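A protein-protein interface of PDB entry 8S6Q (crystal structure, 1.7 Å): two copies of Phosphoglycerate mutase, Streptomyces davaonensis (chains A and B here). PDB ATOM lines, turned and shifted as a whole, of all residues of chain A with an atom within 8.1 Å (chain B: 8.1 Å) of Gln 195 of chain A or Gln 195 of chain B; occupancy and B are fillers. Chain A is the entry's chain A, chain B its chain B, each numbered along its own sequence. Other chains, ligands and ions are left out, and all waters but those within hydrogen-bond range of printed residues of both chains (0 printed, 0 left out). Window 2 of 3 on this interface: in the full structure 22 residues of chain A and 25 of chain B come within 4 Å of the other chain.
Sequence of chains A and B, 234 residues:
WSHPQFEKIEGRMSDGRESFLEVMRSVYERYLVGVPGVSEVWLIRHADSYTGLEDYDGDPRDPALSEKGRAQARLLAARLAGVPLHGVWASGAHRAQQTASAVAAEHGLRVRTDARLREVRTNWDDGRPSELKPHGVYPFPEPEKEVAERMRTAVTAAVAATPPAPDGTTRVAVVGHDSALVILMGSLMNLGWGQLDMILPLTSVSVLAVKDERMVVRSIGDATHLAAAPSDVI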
ATOM      1  N   HIS A 135     -27.752 -22.777 -16.569  1.00  0.00           N
ATOM      2  CA  HIS A 135     -27.246 -21.402 -16.559  1.00  0.00           C
ATOM      3  C   HIS A 135     -25.882 -21.310 -17.223  1.00  0.00           C
ATOM      4  O   HIS A 135     -25.689 -20.563 -18.190  1.00  0.00           O
ATOM      5  CB  HIS A 135     -27.198 -20.883 -15.097  1.00  0.00           C
ATOM      6  CG  HIS A 135     -26.415 -19.606 -14.883  1.00  0.00           C
ATOM      7  ND1 HIS A 135     -25.195 -19.339 -15.471  1.00  0.00           N
ATOM      8  CD2 HIS A 135     -26.698 -18.520 -14.122  1.00  0.00           C
ATOM      9  CE1 HIS A 135     -24.766 -18.149 -15.090  1.00  0.00           C
ATOM     10  NE2 HIS A 135     -25.662 -17.631 -14.269  1.00  0.00           N
ATOM     11  N   GLY A 136     -24.933 -22.071 -16.715  1.00  0.00           N
ATOM     12  CA  GLY A 136     -23.556 -21.931 -17.091  1.00  0.00           C
ATOM     13  C   GLY A 136     -22.661 -21.385 -16.003  1.00  0.00           C
ATOM     14  O   GLY A 136     -21.576 -20.882 -16.325  1.00  0.00           O
ATOM     15  N   GLU A 144     -11.801 -22.730 -12.667  1.00  0.00           N
ATOM     16  CA  GLU A 144     -11.589 -22.621 -14.113  1.00  0.00           C
ATOM     17  C   GLU A 144     -10.230 -22.005 -14.430  1.00  0.00           C
ATOM     18  O   GLU A 144      -9.531 -22.446 -15.377  1.00  0.00           O
ATOM     19  CB  GLU A 144     -12.713 -21.758 -14.696  1.00  0.00           C
ATOM     20  CG  GLU A 144     -12.627 -21.580 -16.197  1.00  0.00           C
ATOM     21  CD  GLU A 144     -13.849 -20.819 -16.718  1.00  0.00           C
ATOM     22  OE1 GLU A 144     -14.649 -20.184 -15.933  1.00  0.00           O
ATOM     23  OE2 GLU A 144     -14.025 -20.848 -17.942  1.00  0.00           O
ATOM     24  N   GLY A 186     -11.827 -21.662 -24.360  1.00  0.00           N
ATOM     25  CA  GLY A 186     -12.630 -20.514 -23.948  1.00  0.00           C
ATOM     26  C   GLY A 186     -11.785 -19.407 -23.335  1.00  0.00           C
ATOM     27  O   GLY A 186     -11.986 -18.223 -23.620  1.00  0.00           O
ATOM     28  N   MET A 189     -10.242 -17.428 -25.986  1.00  0.00           N
ATOM     29  CA  MET A 189     -11.220 -16.721 -26.789  1.00  0.00           C
ATOM     30  C   MET A 189     -11.960 -15.684 -25.959  1.00  0.00           C
ATOM     31  O   MET A 189     -12.848 -15.001 -26.480  1.00  0.00           O
ATOM     32  CB  MET A 189     -12.186 -17.764 -27.331  1.00  0.00           C
ATOM     33  CG  MET A 189     -11.512 -18.655 -28.345  1.00  0.00           C
ATOM     34  SD  MET A 189     -12.665 -19.897 -28.945  1.00  0.00           S
ATOM     35  CE  MET A 189     -13.553 -18.865 -30.051  1.00  0.00           C
ATOM     36  N   ASN A 190     -11.598 -15.564 -24.685  1.00  0.00           N
ATOM     37  CA  ASN A 190     -12.267 -14.651 -23.741  1.00  0.00           C
ATOM     38  C   ASN A 190     -13.759 -14.932 -23.650  1.00  0.00           C
ATOM     39  O   ASN A 190     -14.580 -14.012 -23.632  1.00  0.00           O
ATOM     40  CB  ASN A 190     -12.008 -13.190 -24.114  1.00  0.00           C
ATOM     41  CG  ASN A 190     -10.738 -12.662 -23.468  1.00  0.00           C
ATOM     42  OD1 ASN A 190     -10.732 -12.307 -22.279  1.00  0.00           O
ATOM     43  ND2 ASN A 190      -9.640 -12.660 -24.229  1.00  0.00           N
ATOM     44  N   LEU A 191     -14.100 -16.213 -23.577  1.00  0.00           N
ATOM     45  CA  LEU A 191     -15.463 -16.711 -23.426  1.00  0.00           C
ATOM     46  C   LEU A 191     -15.632 -17.430 -22.093  1.00  0.00           C
ATOM     47  O   LEU A 191     -14.908 -18.399 -21.798  1.00  0.00           O
ATOM     48  CB  LEU A 191     -15.799 -17.677 -24.557  1.00  0.00           C
ATOM     49  CG  LEU A 191     -15.753 -17.034 -25.928  1.00  0.00           C
ATOM     50  CD1 LEU A 191     -16.005 -18.114 -26.961  1.00  0.00           C
ATOM     51  CD2 LEU A 191     -16.854 -15.990 -25.911  1.00  0.00           C
ATOM     52  N   GLY A 192     -16.627 -16.993 -21.327  1.00  0.00           N
ATOM     53  CA  GLY A 192     -16.892 -17.584 -20.033  1.00  0.00           C
ATOM     54  C   GLY A 192     -17.428 -18.986 -20.174  1.00  0.00           C
ATOM     55  O   GLY A 192     -17.864 -19.416 -21.252  1.00  0.00           O
ATOM     56  N   TRP A 193     -17.398 -19.707 -19.054  1.00  0.00           N
ATOM     57  CA  TRP A 193     -17.845 -21.091 -19.042  1.00  0.00           C
ATOM     58  C   TRP A 193     -19.222 -21.223 -19.665  1.00  0.00           C
ATOM     59  O   TRP A 193     -20.162 -20.531 -19.270  1.00  0.00           O
ATOM     60  CB  TRP A 193     -17.888 -21.637 -17.611  1.00  0.00           C
ATOM     61  CG  TRP A 193     -18.561 -22.990 -17.574  1.00  0.00           C
ATOM     62  CD1 TRP A 193     -19.853 -23.264 -17.174  1.00  0.00           C
ATOM     63  CD2 TRP A 193     -18.006 -24.235 -18.023  1.00  0.00           C
ATOM     64  NE1 TRP A 193     -20.097 -24.618 -17.303  1.00  0.00           N
ATOM     65  CE2 TRP A 193     -18.996 -25.227 -17.838  1.00  0.00           C
ATOM     66  CE3 TRP A 193     -16.770 -24.607 -18.544  1.00  0.00           C
ATOM     67  CZ2 TRP A 193     -18.781 -26.556 -18.147  1.00  0.00           C
ATOM     68  CZ3 TRP A 193     -16.552 -25.954 -18.863  1.00  0.00           C
ATOM     69  CH2 TRP A 193     -17.555 -26.907 -18.664  1.00  0.00           C
ATOM     70  N   GLY A 194     -19.337 -22.107 -20.658  1.00  0.00           N
ATOM     71  CA  GLY A 194     -20.625 -22.331 -21.279  1.00  0.00           C
ATOM     72  C   GLY A 194     -20.985 -21.381 -22.408  1.00  0.00           C
ATOM     73  O   GLY A 194     -22.002 -21.599 -23.079  1.00  0.00           O
ATOM     74  N   GLN A 195     -20.207 -20.318 -22.633  1.00  0.00           N
ATOM     75  CA  GLN A 195     -20.447 -19.496 -23.817  1.00  0.00           C
ATOM     76  C   GLN A 195     -20.015 -20.239 -25.069  1.00  0.00           C
ATOM     77  O   GLN A 195     -20.641 -20.135 -26.135  1.00  0.00           O
ATOM     78  CB  GLN A 195     -19.676 -18.199 -23.722  1.00  0.00           C
ATOM     79  CG  GLN A 195     -20.227 -17.331 -22.625  1.00  0.00           C
ATOM     80  CD  GLN A 195     -19.800 -15.898 -22.741  1.00  0.00           C
ATOM     81  OE1 GLN A 195     -18.715 -15.533 -22.309  1.00  0.00           O
ATOM     82  NE2 GLN A 195     -20.637 -15.079 -23.365  1.00  0.00           N
ATOM     83  N   LEU A 196     -18.941 -20.980 -24.961  1.00  0.00           N
ATOM     84  CA  LEU A 196     -18.531 -21.780 -26.089  1.00  0.00           C
ATOM     85  C   LEU A 196     -19.356 -23.049 -25.967  1.00  0.00           C
ATOM     86  O   LEU A 196     -18.922 -24.057 -25.418  1.00  0.00           O
ATOM     87  CB  LEU A 196     -17.037 -22.010 -26.038  1.00  0.00           C
ATOM     88  CG  LEU A 196     -16.328 -22.604 -27.258  1.00  0.00           C
ATOM     89  CD1 LEU A 196     -16.412 -21.755 -28.540  1.00  0.00           C
ATOM     90  CD2 LEU A 196     -14.881 -22.814 -26.821  1.00  0.00           C
ATOM     91  N   ASP A 197     -20.570 -22.989 -26.487  1.00  0.00           N
ATOM     92  CA  ASP A 197     -21.582 -23.998 -26.203  1.00  0.00           C
ATOM     93  C   ASP A 197     -21.470 -25.138 -27.210  1.00  0.00           C
ATOM     94  O   ASP A 197     -22.303 -25.318 -28.096  1.00  0.00           O
ATOM     95  CB  ASP A 197     -22.964 -23.372 -26.222  1.00  0.00           C
ATOM     96  CG  ASP A 197     -24.027 -24.326 -25.752  1.00  0.00           C
ATOM     97  OD1 ASP A 197     -23.699 -25.155 -24.876  1.00  0.00           O
ATOM     98  OD2 ASP A 197     -25.181 -24.220 -26.227  1.00  0.00           O
ATOM     99  N   MET A 198     -20.417 -25.921 -27.042  1.00  0.00           N
ATOM    100  CA  MET A 198     -20.262 -27.101 -27.878  1.00  0.00           C
ATOM    101  C   MET A 198     -19.533 -28.161 -27.087  1.00  0.00           C
ATOM    102  O   MET A 198     -18.790 -27.876 -26.133  1.00  0.00           O
ATOM    103  CB  MET A 198     -19.487 -26.836 -29.175  1.00  0.00           C
ATOM    104  CG  MET A 198     -18.312 -25.883 -29.034  1.00  0.00           C
ATOM    105  SD  MET A 198     -17.737 -25.196 -30.616  1.00  0.00           S
ATOM    106  CE  MET A 198     -17.943 -26.618 -31.685  1.00  0.00           C
ATOM    107  N   GLY B 136     -17.503  -6.311 -29.868  1.00  0.00           N
ATOM    108  CA  GLY B 136     -17.137  -5.326 -30.868  1.00  0.00           C
ATOM    109  C   GLY B 136     -18.337  -4.774 -31.615  1.00  0.00           C
ATOM    110  O   GLY B 136     -19.408  -5.383 -31.608  1.00  0.00           O
ATOM    111  N   GLU B 144     -26.953  -7.675 -38.661  1.00  0.00           N
ATOM    112  CA  GLU B 144     -26.499  -9.014 -38.296  1.00  0.00           C
ATOM    113  C   GLU B 144     -27.632 -10.030 -38.360  1.00  0.00           C
ATOM    114  O   GLU B 144     -27.449 -11.157 -38.842  1.00  0.00           O
ATOM    115  CB  GLU B 144     -25.923  -8.966 -36.886  1.00  0.00           C
ATOM    116  CG  GLU B 144     -25.326 -10.280 -36.433  1.00  0.00           C
ATOM    117  CD  GLU B 144     -24.409 -10.064 -35.249  1.00  0.00           C
ATOM    118  OE1 GLU B 144     -24.559  -9.000 -34.627  1.00  0.00           O
ATOM    119  OE2 GLU B 144     -23.545 -10.923 -34.965  1.00  0.00           O
ATOM    120  N   VAL B 182     -19.611 -16.895 -40.288  1.00  0.00           N
ATOM    121  CA  VAL B 182     -19.355 -16.728 -38.842  1.00  0.00           C
ATOM    122  C   VAL B 182     -20.577 -16.138 -38.151  1.00  0.00           C
ATOM    123  O   VAL B 182     -20.838 -16.418 -36.959  1.00  0.00           O
ATOM    124  CB  VAL B 182     -18.107 -15.859 -38.595  1.00  0.00           C
ATOM    125  CG1 VAL B 182     -17.900 -15.620 -37.129  1.00  0.00           C
ATOM    126  CG2 VAL B 182     -16.854 -16.569 -39.110  1.00  0.00           C
ATOM    127  N   GLY B 186     -22.251 -17.913 -35.044  1.00  0.00           N
ATOM    128  CA  GLY B 186     -22.390 -17.155 -33.799  1.00  0.00           C
ATOM    129  C   GLY B 186     -23.832 -17.090 -33.335  1.00  0.00           C
ATOM    130  O   GLY B 186     -24.137 -17.352 -32.173  1.00  0.00           O
ATOM    131  N   MET B 189     -25.068 -20.145 -31.659  1.00  0.00           N
ATOM    132  CA  MET B 189     -24.528 -20.343 -30.321  1.00  0.00           C
ATOM    133  C   MET B 189     -24.860 -19.177 -29.426  1.00  0.00           C
ATOM    134  O   MET B 189     -24.272 -19.063 -28.351  1.00  0.00           O
ATOM    135  CB  MET B 189     -23.004 -20.531 -30.373  1.00  0.00           C
ATOM    136  CG  MET B 189     -22.518 -21.130 -31.666  1.00  0.00           C
ATOM    137  SD  MET B 189     -20.727 -21.413 -31.930  1.00  0.00           S
ATOM    138  CE  MET B 189     -20.429 -22.501 -30.572  1.00  0.00           C
ATOM    139  N   ASN B 190     -25.735 -18.276 -29.877  1.00  0.00           N
ATOM    140  CA  ASN B 190     -26.129 -17.122 -29.060  1.00  0.00           C
ATOM    141  C   ASN B 190     -24.889 -16.316 -28.691  1.00  0.00           C
ATOM    142  O   ASN B 190     -24.693 -15.934 -27.534  1.00  0.00           O
ATOM    143  CB  ASN B 190     -26.868 -17.549 -27.786  1.00  0.00           C
ATOM    144  CG  ASN B 190     -28.198 -18.203 -28.076  1.00  0.00           C
ATOM    145  OD1 ASN B 190     -28.302 -19.430 -28.068  1.00  0.00           O
ATOM    146  ND2 ASN B 190     -29.211 -17.395 -28.396  1.00  0.00           N
ATOM    147  N   LEU B 191     -23.987 -16.164 -29.656  1.00  0.00           N
ATOM    148  CA  LEU B 191     -22.858 -15.255 -29.548  1.00  0.00           C
ATOM    149  C   LEU B 191     -23.046 -14.094 -30.519  1.00  0.00           C
ATOM    150  O   LEU B 191     -23.537 -14.275 -31.630  1.00  0.00           O
ATOM    151  CB  LEU B 191     -21.546 -15.974 -29.813  1.00  0.00           C
ATOM    152  CG  LEU B 191     -21.314 -17.187 -28.903  1.00  0.00           C
ATOM    153  CD1 LEU B 191     -19.946 -17.874 -29.243  1.00  0.00           C
ATOM    154  CD2 LEU B 191     -21.422 -16.774 -27.415  1.00  0.00           C
ATOM    155  N   GLY B 192     -22.718 -12.897 -30.068  1.00  0.00           N
ATOM    156  CA  GLY B 192     -22.802 -11.749 -30.936  1.00  0.00           C
ATOM    157  C   GLY B 192     -21.539 -11.593 -31.727  1.00  0.00           C
ATOM    158  O   GLY B 192     -20.535 -12.261 -31.466  1.00  0.00           O
ATOM    159  N   TRP B 193     -21.597 -10.707 -32.718  1.00  0.00           N
ATOM    160  CA  TRP B 193     -20.426 -10.459 -33.551  1.00  0.00           C
ATOM    161  C   TRP B 193     -19.264 -10.036 -32.665  1.00  0.00           C
ATOM    162  O   TRP B 193     -19.411  -9.173 -31.792  1.00  0.00           O
ATOM    163  CB  TRP B 193     -20.732  -9.382 -34.597  1.00  0.00           C
ATOM    164  CG  TRP B 193     -19.560  -8.973 -35.421  1.00  0.00           C
ATOM    165  CD1 TRP B 193     -18.738  -7.888 -35.218  1.00  0.00           C
ATOM    166  CD2 TRP B 193     -19.096  -9.611 -36.606  1.00  0.00           C
ATOM    167  NE1 TRP B 193     -17.770  -7.840 -36.202  1.00  0.00           N
ATOM    168  CE2 TRP B 193     -17.976  -8.886 -37.067  1.00  0.00           C
ATOM    169  CE3 TRP B 193     -19.510 -10.737 -37.318  1.00  0.00           C
ATOM    170  CZ2 TRP B 193     -17.273  -9.249 -38.202  1.00  0.00           C
ATOM    171  CZ3 TRP B 193     -18.794 -11.108 -38.458  1.00  0.00           C
ATOM    172  CH2 TRP B 193     -17.695 -10.362 -38.886  1.00  0.00           C
ATOM    173  N   GLY B 194     -18.116 -10.682 -32.862  1.00  0.00           N
ATOM    174  CA  GLY B 194     -16.950 -10.454 -32.054  1.00  0.00           C
ATOM    175  C   GLY B 194     -16.743 -11.444 -30.916  1.00  0.00           C
ATOM    176  O   GLY B 194     -15.601 -11.636 -30.492  1.00  0.00           O
ATOM    177  N   GLN B 195     -17.806 -12.065 -30.395  1.00  0.00           N
ATOM    178  CA  GLN B 195     -17.623 -13.023 -29.303  1.00  0.00           C
ATOM    179  C   GLN B 195     -17.002 -14.309 -29.800  1.00  0.00           C
ATOM    180  O   GLN B 195     -16.106 -14.853 -29.153  1.00  0.00           O
ATOM    181  CB  GLN B 195     -18.954 -13.322 -28.626  1.00  0.00           C
ATOM    182  CG  GLN B 195     -19.642 -12.114 -28.086  1.00  0.00           C
ATOM    183  CD  GLN B 195     -20.598 -12.476 -27.008  1.00  0.00           C
ATOM    184  OE1 GLN B 195     -21.797 -12.575 -27.278  1.00  0.00           O
ATOM    185  NE2 GLN B 195     -20.108 -12.673 -25.781  1.00  0.00           N
ATOM    186  N   LEU B 196     -17.493 -14.818 -30.928  1.00  0.00           N
ATOM    187  CA  LEU B 196     -16.831 -15.888 -31.654  1.00  0.00           C
ATOM    188  C   LEU B 196     -15.708 -15.219 -32.435  1.00  0.00           C
ATOM    189  O   LEU B 196     -15.861 -14.826 -33.595  1.00  0.00           O
ATOM    190  CB  LEU B 196     -17.811 -16.608 -32.573  1.00  0.00           C
ATOM    191  CG  LEU B 196     -17.275 -17.969 -32.991  1.00  0.00           C
ATOM    192  CD1 LEU B 196     -17.099 -18.764 -31.735  1.00  0.00           C
ATOM    193  CD2 LEU B 196     -18.191 -18.685 -33.964  1.00  0.00           C
ATOM    194  N   ASP B 197     -14.574 -15.036 -31.763  1.00  0.00           N
ATOM    195  CA  ASP B 197     -13.504 -14.206 -32.312  1.00  0.00           C
ATOM    196  C   ASP B 197     -12.537 -15.081 -33.118  1.00  0.00           C
ATOM    197  O   ASP B 197     -11.393 -15.324 -32.753  1.00  0.00           O
ATOM    198  CB  ASP B 197     -12.836 -13.416 -31.195  1.00  0.00           C
ATOM    199  CG  ASP B 197     -11.577 -12.720 -31.640  1.00  0.00           C
ATOM    200  OD1 ASP B 197     -11.662 -11.918 -32.592  1.00  0.00           O
ATOM    201  OD2 ASP B 197     -10.534 -12.880 -30.961  1.00  0.00           O
ATOM    202  N   MET B 198     -13.040 -15.521 -34.261  1.00  0.00           N
ATOM    203  CA  MET B 198     -12.261 -16.335 -35.188  1.00  0.00           C
ATOM    204  C   MET B 198     -12.455 -15.890 -36.641  1.00  0.00           C
ATOM    205  O   MET B 198     -13.525 -15.389 -37.018  1.00  0.00           O
ATOM    206  CB  MET B 198     -12.608 -17.826 -35.111  1.00  0.00           C
ATOM    207  CG  MET B 198     -12.403 -18.642 -33.811  1.00  0.00           C
ATOM    208  SD  MET B 198     -13.639 -19.978 -33.841  1.00  0.00           S
ATOM    209  CE  MET B 198     -12.498 -21.260 -34.524  1.00  0.00           C
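O of Gly 186 of chain A lies within hydrogen-bond range of N of Leu 191 of chain A (2.9 Å). The backbone NH of Gly 192 of chain A sits at hydrogen-bond distance from the side-chain amide oxygen of Gln 195 of chain A (2.7 Å). The backbone carbonyl oxygen of Gly 186 of chain B sits at hydrogen-bond distance from the backbone NH of Leu 191 of chain B (2.8 Å). N of Gly 192 of chain B is in hydrogen-bond range of OE1 of Gln 195 of chain B (3.0 Å).
Gln 195 of chain A touches just these residues of chain B: Leu 191 and Gln 195. Of the printed residues of chain A, Gln 195 of chain B touches Leu 191 and Gln 195. No residue of chain B comes within 4 Å of Gly 194 of chain A. No residue of chain A comes within 4 Å of Gly 192 of chain B. No residue of chain A comes within 4 Å of Gly 194 of chain B. Printed residues of chain A within 4 Å of Leu 191 of chain B: Gln 195. Printed residues of chain A within 4 Å of Met 198 of chain B: Met 189 (3.9 Å). Printed residues of chain B within 4 Å of Met 189 of chain A: Leu 196 and Met 198. Of the printed residues of chain A, Met 189 of chain B touches Met 198. Of the printed residues of chain B, Met 198 of chain A touches Met 189 (3.8 Å). The nearest residue of chain B that does not touch Gln 195 of chain A is Met 189 of chain B (4.4 Å). The nearest printed residue of chain A that does not touch Leu 191 of chain B is Leu 191 of chain A (4.6 Å).
Hydrophobic or aromatic side chains of chain A that line the printed part of chain B: Met 189, Leu 191 and Met 198. Of the 14 printed residues of chain B, 5 touch a printed residue of chain A. Hydrophobic or aromatic side chains of chain B within 4 Å of the printed part of chain A: Met 189, Leu 191, Leu 196 and Met 198. Among the printed residues, 6 pairs touch across the chains. Among the printed residues, no Asp or Glu carboxylate lies within 4 Å of a Lys or Arg side-chain nitrogen of the other chain.
The side-chain amide nitrogen (NE2) of Gln 195 of chain A sits close to the side-chain amide nitrogen (NE2) of Gln 195 of chain B, 3.5 Å away.
Met 189 of chain A touches Leu 196 of chain B, but with the chains exchanged Leu 196 of chain A does not touch Met 189 of chain B (4.6 Å). Met 189 of chain A touches Met 198 of chain B, and with the chains exchanged Met 198 of chain A touches Met 189 of chain B. Leu 191 of chain A touches Gln 195 of chain B, and with the chains exchanged Gln 195 of chain A touches Leu 191 of chain B. Gln 195 of chain A touches its own counterpart, Gln 195 of chain B. 13 positions are printed for both chains.
Leu 196 of chain B touches Met 189 of chain A (CD1 to CE, 3.9 Å). Met 189 of chain A touches Met 198 of chain B (CE to CG, 3.9 Å). CD2 of Leu 191 of chain A touches O of Gln 195 of chain B, 3.5 Å away. Gln 195 of chain A touches Leu 191 of chain B. SD of Met 198 of chain A touches CE of Met 189 of chain B, 3.8 Å away.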
